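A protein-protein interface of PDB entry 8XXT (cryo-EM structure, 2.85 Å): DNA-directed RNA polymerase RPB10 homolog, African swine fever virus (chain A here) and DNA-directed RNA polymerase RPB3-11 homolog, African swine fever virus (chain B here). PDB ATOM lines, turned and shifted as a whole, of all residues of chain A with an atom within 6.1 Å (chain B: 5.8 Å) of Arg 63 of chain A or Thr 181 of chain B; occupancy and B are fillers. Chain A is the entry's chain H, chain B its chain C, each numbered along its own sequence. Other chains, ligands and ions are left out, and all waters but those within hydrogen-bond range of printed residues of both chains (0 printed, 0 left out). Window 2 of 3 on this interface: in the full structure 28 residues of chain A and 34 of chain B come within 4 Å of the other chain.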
ATOM      1  N   CYS A  10      14.896 -35.208  -3.773  1.00  0.00           N
ATOM      2  CA  CYS A  10      13.626 -35.126  -4.476  1.00  0.00           C
ATOM      3  C   CYS A  10      13.753 -34.956  -5.980  1.00  0.00           C
ATOM      4  O   CYS A  10      12.792 -35.256  -6.696  1.00  0.00           O
ATOM      5  CB  CYS A  10      12.782 -33.973  -3.922  1.00  0.00           C
ATOM      6  SG  CYS A  10      13.219 -32.369  -4.596  1.00  0.00           S
ATOM      7  N   PHE A  12      14.490 -32.014  -7.679  1.00  0.00           N
ATOM      8  CA  PHE A  12      14.256 -30.680  -8.207  1.00  0.00           C
ATOM      9  C   PHE A  12      15.537 -30.161  -8.850  1.00  0.00           C
ATOM     10  O   PHE A  12      16.610 -30.260  -8.247  1.00  0.00           O
ATOM     11  CB  PHE A  12      13.797 -29.738  -7.104  1.00  0.00           C
ATOM     12  CG  PHE A  12      13.318 -28.414  -7.608  1.00  0.00           C
ATOM     13  CD1 PHE A  12      12.032 -28.269  -8.088  1.00  0.00           C
ATOM     14  CD2 PHE A  12      14.155 -27.316  -7.611  1.00  0.00           C
ATOM     15  CE1 PHE A  12      11.590 -27.056  -8.557  1.00  0.00           C
ATOM     16  CE2 PHE A  12      13.715 -26.100  -8.079  1.00  0.00           C
ATOM     17  CZ  PHE A  12      12.431 -25.970  -8.551  1.00  0.00           C
ATOM     18  N   ILE A  60      13.946 -21.475  -6.145  1.00  0.00           N
ATOM     19  CA  ILE A  60      13.950 -22.724  -5.390  1.00  0.00           C
ATOM     20  C   ILE A  60      12.884 -22.625  -4.306  1.00  0.00           C
ATOM     21  O   ILE A  60      12.892 -21.673  -3.514  1.00  0.00           O
ATOM     22  CB  ILE A  60      15.331 -23.024  -4.791  1.00  0.00           C
ATOM     23  CG1 ILE A  60      16.303 -23.472  -5.879  1.00  0.00           C
ATOM     24  CG2 ILE A  60      15.226 -24.087  -3.713  1.00  0.00           C
ATOM     25  CD1 ILE A  60      17.277 -22.412  -6.294  1.00  0.00           C
ATOM     26  N   PRO A  61      11.954 -23.570  -4.235  1.00  0.00           N
ATOM     27  CA  PRO A  61      10.890 -23.483  -3.228  1.00  0.00           C
ATOM     28  C   PRO A  61      11.412 -23.685  -1.818  1.00  0.00           C
ATOM     29  O   PRO A  61      12.606 -23.913  -1.615  1.00  0.00           O
ATOM     30  CB  PRO A  61       9.927 -24.603  -3.639  1.00  0.00           C
ATOM     31  CG  PRO A  61      10.774 -25.561  -4.398  1.00  0.00           C
ATOM     32  CD  PRO A  61      11.799 -24.743  -5.108  1.00  0.00           C
ATOM     33  N   MET A  62      10.520 -23.607  -0.835  1.00  0.00           N
ATOM     34  CA  MET A  62      10.910 -23.767   0.558  1.00  0.00           C
ATOM     35  C   MET A  62      11.078 -25.240   0.899  1.00  0.00           C
ATOM     36  O   MET A  62      10.470 -25.735   1.854  1.00  0.00           O
ATOM     37  CB  MET A  62       9.872 -23.126   1.478  1.00  0.00           C
ATOM     38  CG  MET A  62      10.452 -22.419   2.682  1.00  0.00           C
ATOM     39  SD  MET A  62      11.959 -21.524   2.294  1.00  0.00           S
ATOM     40  CE  MET A  62      12.453 -21.008   3.930  1.00  0.00           C
ATOM     41  N   ARG A  63      11.897 -25.946   0.131  1.00  0.00           N
ATOM     42  CA  ARG A  63      12.111 -27.372   0.316  1.00  0.00           C
ATOM     43  C   ARG A  63      13.367 -27.586   1.143  1.00  0.00           C
ATOM     44  O   ARG A  63      14.425 -27.041   0.821  1.00  0.00           O
ATOM     45  CB  ARG A  63      12.235 -28.084  -1.029  1.00  0.00           C
ATOM     46  CG  ARG A  63      10.944 -28.131  -1.815  1.00  0.00           C
ATOM     47  CD  ARG A  63      11.113 -28.899  -3.110  1.00  0.00           C
ATOM     48  NE  ARG A  63      11.106 -30.341  -2.898  1.00  0.00           N
ATOM     49  CZ  ARG A  63      10.024 -31.056  -2.632  1.00  0.00           C
ATOM     50  NH1 ARG A  63       8.832 -30.495  -2.529  1.00  0.00           N
ATOM     51  NH2 ARG A  63      10.139 -32.370  -2.467  1.00  0.00           N
ATOM     52  N   VAL A  64      13.245 -28.378   2.208  1.00  0.00           N
ATOM     53  CA  VAL A  64      14.386 -28.626   3.082  1.00  0.00           C
ATOM     54  C   VAL A  64      15.524 -29.260   2.299  1.00  0.00           C
ATOM     55  O   VAL A  64      16.691 -28.886   2.458  1.00  0.00           O
ATOM     56  CB  VAL A  64      13.964 -29.507   4.271  1.00  0.00           C
ATOM     57  CG1 VAL A  64      15.182 -29.998   5.025  1.00  0.00           C
ATOM     58  CG2 VAL A  64      13.034 -28.741   5.191  1.00  0.00           C
ATOM     59  N   CYS A  65      15.201 -30.216   1.432  1.00  0.00           N
ATOM     60  CA  CYS A  65      16.231 -30.964   0.722  1.00  0.00           C
ATOM     61  C   CYS A  65      17.008 -30.077  -0.238  1.00  0.00           C
ATOM     62  O   CYS A  65      18.242 -30.069  -0.230  1.00  0.00           O
ATOM     63  CB  CYS A  65      15.593 -32.127  -0.028  1.00  0.00           C
ATOM     64  SG  CYS A  65      14.103 -31.703  -0.939  1.00  0.00           S
ATOM     65  N   CYS A  66      16.298 -29.323  -1.079  1.00  0.00           N
ATOM     66  CA  CYS A  66      16.959 -28.554  -2.126  1.00  0.00           C
ATOM     67  C   CYS A  66      17.854 -27.471  -1.543  1.00  0.00           C
ATOM     68  O   CYS A  66      18.958 -27.236  -2.041  1.00  0.00           O
ATOM     69  CB  CYS A  66      15.917 -27.950  -3.061  1.00  0.00           C
ATOM     70  SG  CYS A  66      14.792 -29.174  -3.741  1.00  0.00           S
ATOM     71  N   ARG A  67      17.392 -26.796  -0.491  1.00  0.00           N
ATOM     72  CA  ARG A  67      18.228 -25.793   0.156  1.00  0.00           C
ATOM     73  C   ARG A  67      19.403 -26.435   0.875  1.00  0.00           C
ATOM     74  O   ARG A  67      20.492 -25.855   0.935  1.00  0.00           O
ATOM     75  CB  ARG A  67      17.394 -24.966   1.127  1.00  0.00           C
ATOM     76  CG  ARG A  67      16.141 -24.414   0.504  1.00  0.00           C
ATOM     77  CD  ARG A  67      15.813 -23.057   1.055  1.00  0.00           C
ATOM     78  NE  ARG A  67      14.880 -22.357   0.187  1.00  0.00           N
ATOM     79  CZ  ARG A  67      14.620 -21.061   0.263  1.00  0.00           C
ATOM     80  NH1 ARG A  67      15.206 -20.293   1.165  1.00  0.00           N
ATOM     81  NH2 ARG A  67      13.751 -20.523  -0.587  1.00  0.00           N
ATOM     82  N   THR A  68      19.202 -27.626   1.439  1.00  0.00           N
ATOM     83  CA  THR A  68      20.289 -28.318   2.120  1.00  0.00           C
ATOM     84  C   THR A  68      21.416 -28.654   1.155  1.00  0.00           C
ATOM     85  O   THR A  68      22.592 -28.415   1.448  1.00  0.00           O
ATOM     86  CB  THR A  68      19.763 -29.587   2.780  1.00  0.00           C
ATOM     87  OG1 THR A  68      18.856 -29.240   3.828  1.00  0.00           O
ATOM     88  CG2 THR A  68      20.894 -30.379   3.356  1.00  0.00           C
ATOM     89  N   ASN B  41       4.779 -25.577 -10.443  1.00  0.00           N
ATOM     90  CA  ASN B  41       4.078 -26.230  -9.347  1.00  0.00           C
ATOM     91  C   ASN B  41       2.595 -26.288  -9.678  1.00  0.00           C
ATOM     92  O   ASN B  41       1.933 -25.249  -9.764  1.00  0.00           O
ATOM     93  CB  ASN B  41       4.310 -25.487  -8.035  1.00  0.00           C
ATOM     94  CG  ASN B  41       3.803 -26.254  -6.836  1.00  0.00           C
ATOM     95  OD1 ASN B  41       4.231 -27.374  -6.576  1.00  0.00           O
ATOM     96  ND2 ASN B  41       2.887 -25.653  -6.095  1.00  0.00           N
ATOM     97  N   VAL B  42       2.075 -27.496  -9.857  1.00  0.00           N
ATOM     98  CA  VAL B  42       0.676 -27.716 -10.196  1.00  0.00           C
ATOM     99  C   VAL B  42      -0.023 -28.271  -8.968  1.00  0.00           C
ATOM    100  O   VAL B  42       0.273 -29.388  -8.527  1.00  0.00           O
ATOM    101  CB  VAL B  42       0.531 -28.668 -11.390  1.00  0.00           C
ATOM    102  CG1 VAL B  42      -0.925 -28.944 -11.665  1.00  0.00           C
ATOM    103  CG2 VAL B  42       1.196 -28.073 -12.611  1.00  0.00           C
ATOM    104  N   VAL B  43      -0.947 -27.494  -8.413  1.00  0.00           N
ATOM    105  CA  VAL B  43      -1.735 -27.897  -7.255  1.00  0.00           C
ATOM    106  C   VAL B  43      -3.155 -28.163  -7.726  1.00  0.00           C
ATOM    107  O   VAL B  43      -3.767 -27.314  -8.384  1.00  0.00           O
ATOM    108  CB  VAL B  43      -1.709 -26.829  -6.150  1.00  0.00           C
ATOM    109  CG1 VAL B  43      -2.535 -27.283  -4.976  1.00  0.00           C
ATOM    110  CG2 VAL B  43      -0.286 -26.558  -5.716  1.00  0.00           C
ATOM    111  N   VAL B 179       7.863 -34.022  -8.893  1.00  0.00           N
ATOM    112  CA  VAL B 179       8.308 -34.054  -7.506  1.00  0.00           C
ATOM    113  C   VAL B 179       7.149 -33.624  -6.619  1.00  0.00           C
ATOM    114  O   VAL B 179       6.382 -32.720  -6.972  1.00  0.00           O
ATOM    115  CB  VAL B 179       9.555 -33.171  -7.297  1.00  0.00           C
ATOM    116  CG1 VAL B 179       9.956 -32.499  -8.594  1.00  0.00           C
ATOM    117  CG2 VAL B 179       9.330 -32.135  -6.210  1.00  0.00           C
ATOM    118  N   LYS B 180       6.998 -34.298  -5.482  1.00  0.00           N
ATOM    119  CA  LYS B 180       5.877 -34.035  -4.591  1.00  0.00           C
ATOM    120  C   LYS B 180       6.084 -32.732  -3.836  1.00  0.00           C
ATOM    121  O   LYS B 180       7.148 -32.499  -3.258  1.00  0.00           O
ATOM    122  CB  LYS B 180       5.709 -35.186  -3.605  1.00  0.00           C
ATOM    123  CG  LYS B 180       5.247 -36.477  -4.240  1.00  0.00           C
ATOM    124  CD  LYS B 180       5.171 -37.594  -3.226  1.00  0.00           C
ATOM    125  CE  LYS B 180       6.549 -37.955  -2.709  1.00  0.00           C
ATOM    126  NZ  LYS B 180       7.468 -38.378  -3.794  1.00  0.00           N
ATOM    127  N   THR B 181       5.062 -31.874  -3.846  1.00  0.00           N
ATOM    128  CA  THR B 181       5.089 -30.641  -3.077  1.00  0.00           C
ATOM    129  C   THR B 181       3.909 -30.475  -2.137  1.00  0.00           C
ATOM    130  O   THR B 181       3.999 -29.663  -1.211  1.00  0.00           O
ATOM    131  CB  THR B 181       5.142 -29.415  -4.001  1.00  0.00           C
ATOM    132  OG1 THR B 181       3.820 -29.094  -4.448  1.00  0.00           O
ATOM    133  CG2 THR B 181       6.031 -29.680  -5.198  1.00  0.00           C
ATOM    134  N   HIS B 182       2.814 -31.200  -2.338  1.00  0.00           N
ATOM    135  CA  HIS B 182       1.682 -31.108  -1.429  1.00  0.00           C
ATOM    136  C   HIS B 182       0.801 -32.336  -1.575  1.00  0.00           C
ATOM    137  O   HIS B 182       0.652 -32.886  -2.669  1.00  0.00           O
ATOM    138  CB  HIS B 182       0.855 -29.844  -1.674  1.00  0.00           C
ATOM    139  CG  HIS B 182      -0.148 -29.572  -0.602  1.00  0.00           C
ATOM    140  ND1 HIS B 182       0.141 -28.823   0.517  1.00  0.00           N
ATOM    141  CD2 HIS B 182      -1.439 -29.958  -0.473  1.00  0.00           C
ATOM    142  CE1 HIS B 182      -0.929 -28.757   1.289  1.00  0.00           C
ATOM    143  NE2 HIS B 182      -1.901 -29.437   0.710  1.00  0.00           N
ATOM    144  N   PHE B 183       0.223 -32.755  -0.452  1.00  0.00           N
ATOM    145  CA  PHE B 183      -0.810 -33.786  -0.442  1.00  0.00           C
ATOM    146  C   PHE B 183      -1.580 -33.660   0.859  1.00  0.00           C
ATOM    147  O   PHE B 183      -0.998 -33.806   1.937  1.00  0.00           O
ATOM    148  CB  PHE B 183      -0.215 -35.178  -0.572  1.00  0.00           C
ATOM    149  CG  PHE B 183      -1.245 -36.260  -0.706  1.00  0.00           C
ATOM    150  CD1 PHE B 183      -2.200 -36.203  -1.705  1.00  0.00           C
ATOM    151  CD2 PHE B 183      -1.267 -37.327   0.169  1.00  0.00           C
ATOM    152  CE1 PHE B 183      -3.147 -37.194  -1.829  1.00  0.00           C
ATOM    153  CE2 PHE B 183      -2.212 -38.318   0.047  1.00  0.00           C
ATOM    154  CZ  PHE B 183      -3.153 -38.252  -0.950  1.00  0.00           C
ATOM    155  N   GLY B 219      -0.445 -31.649  -4.800  1.00  0.00           N
ATOM    156  CA  GLY B 219       0.486 -30.697  -5.370  1.00  0.00           C
ATOM    157  C   GLY B 219       1.712 -31.358  -5.957  1.00  0.00           C
ATOM    158  O   GLY B 219       2.404 -32.114  -5.272  1.00  0.00           O
ATOM    159  N   LEU B 220       1.995 -31.081  -7.224  1.00  0.00           N
ATOM    160  CA  LEU B 220       3.131 -31.664  -7.916  1.00  0.00           C
ATOM    161  C   LEU B 220       3.898 -30.574  -8.642  1.00  0.00           C
ATOM    162  O   LEU B 220       3.328 -29.561  -9.051  1.00  0.00           O
ATOM    163  CB  LEU B 220       2.690 -32.732  -8.913  1.00  0.00           C
ATOM    164  CG  LEU B 220       2.270 -34.081  -8.341  1.00  0.00           C
ATOM    165  CD1 LEU B 220       1.725 -34.945  -9.443  1.00  0.00           C
ATOM    166  CD2 LEU B 220       3.438 -34.764  -7.666  1.00  0.00           C
ATOM    167  N   CYS B 221       5.200 -30.787  -8.800  1.00  0.00           N
ATOM    168  CA  CYS B 221       6.072 -29.853  -9.497  1.00  0.00           C
ATOM    169  C   CYS B 221       6.733 -30.558 -10.669  1.00  0.00           C
ATOM    170  O   CYS B 221       7.335 -31.620 -10.500  1.00  0.00           O
ATOM    171  CB  CYS B 221       7.134 -29.280  -8.559  1.00  0.00           C
ATOM    172  SG  CYS B 221       8.310 -28.173  -9.348  1.00  0.00           S
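Printed residues of chain B within 4 Å of Phe 12 of chain A: Cys 221 (3.6 Å). Of the printed residues of chain B, Arg 63 of chain A touches Val 179, Lys 180 and Thr 181. Of the printed residues of chain A, Lys 180 of chain B touches Arg 63. Thr 181 of chain B touches just one residue of chain A: Arg 63 (3.8 Å). The nearest printed residue of chain B that does not touch Arg 63 of chain A is His 182 of chain B (6.1 Å). The nearest printed residue of chain A that does not touch Thr 181 of chain B is Pro 61 of chain A (6.3 Å).
Printed residues of chain B that touch a printed residue of chain A: Val 179, Lys 180, Thr 181 and Cys 221. Hydrophobic or aromatic side chains of chain B that line the printed part of chain A: Val 179. Among the printed residues, 5 pairs touch across the chains.
The side-chain amide oxygen (OD1) of Asn 41 of chain B sits at hydrogen-bond distance from the side-chain hydroxyl (OG1) of Thr 181 of chain B. The backbone carbonyl oxygen of Val 179 of chain B sits at hydrogen-bond distance from the backbone NH of Cys 221 of chain B, at 2.9 Å. N of Thr 181 of chain B is in hydrogen-bond range of O of Gly 219 of chain B (3.0 Å). SG of Cys 10 of chain A lies close to N of Phe 12 of chain A, at 3.4 Å. The side-chain sulfur (SG) of Cys 10 of chain A lies close to the guanidinium group (NE) of Arg 63 of chain A (3.4 Å).
The backbone carbonyl oxygen of Lys 180 of chain B is in hydrogen-bond range of the guanidinium group of Arg 63 of chain A.
Cys 10 of chain A touches Val 179 of chain B (O to CB, 3.9 Å). Phe 12 of chain A touches Cys 221 of chain B (CE1 to SG, 3.6 Å). Val 179 of chain B touches Arg 63 of chain A (CG2 to CZ, 3.8 Å). Arg 63 of chain A touches Thr 181 of chain B.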
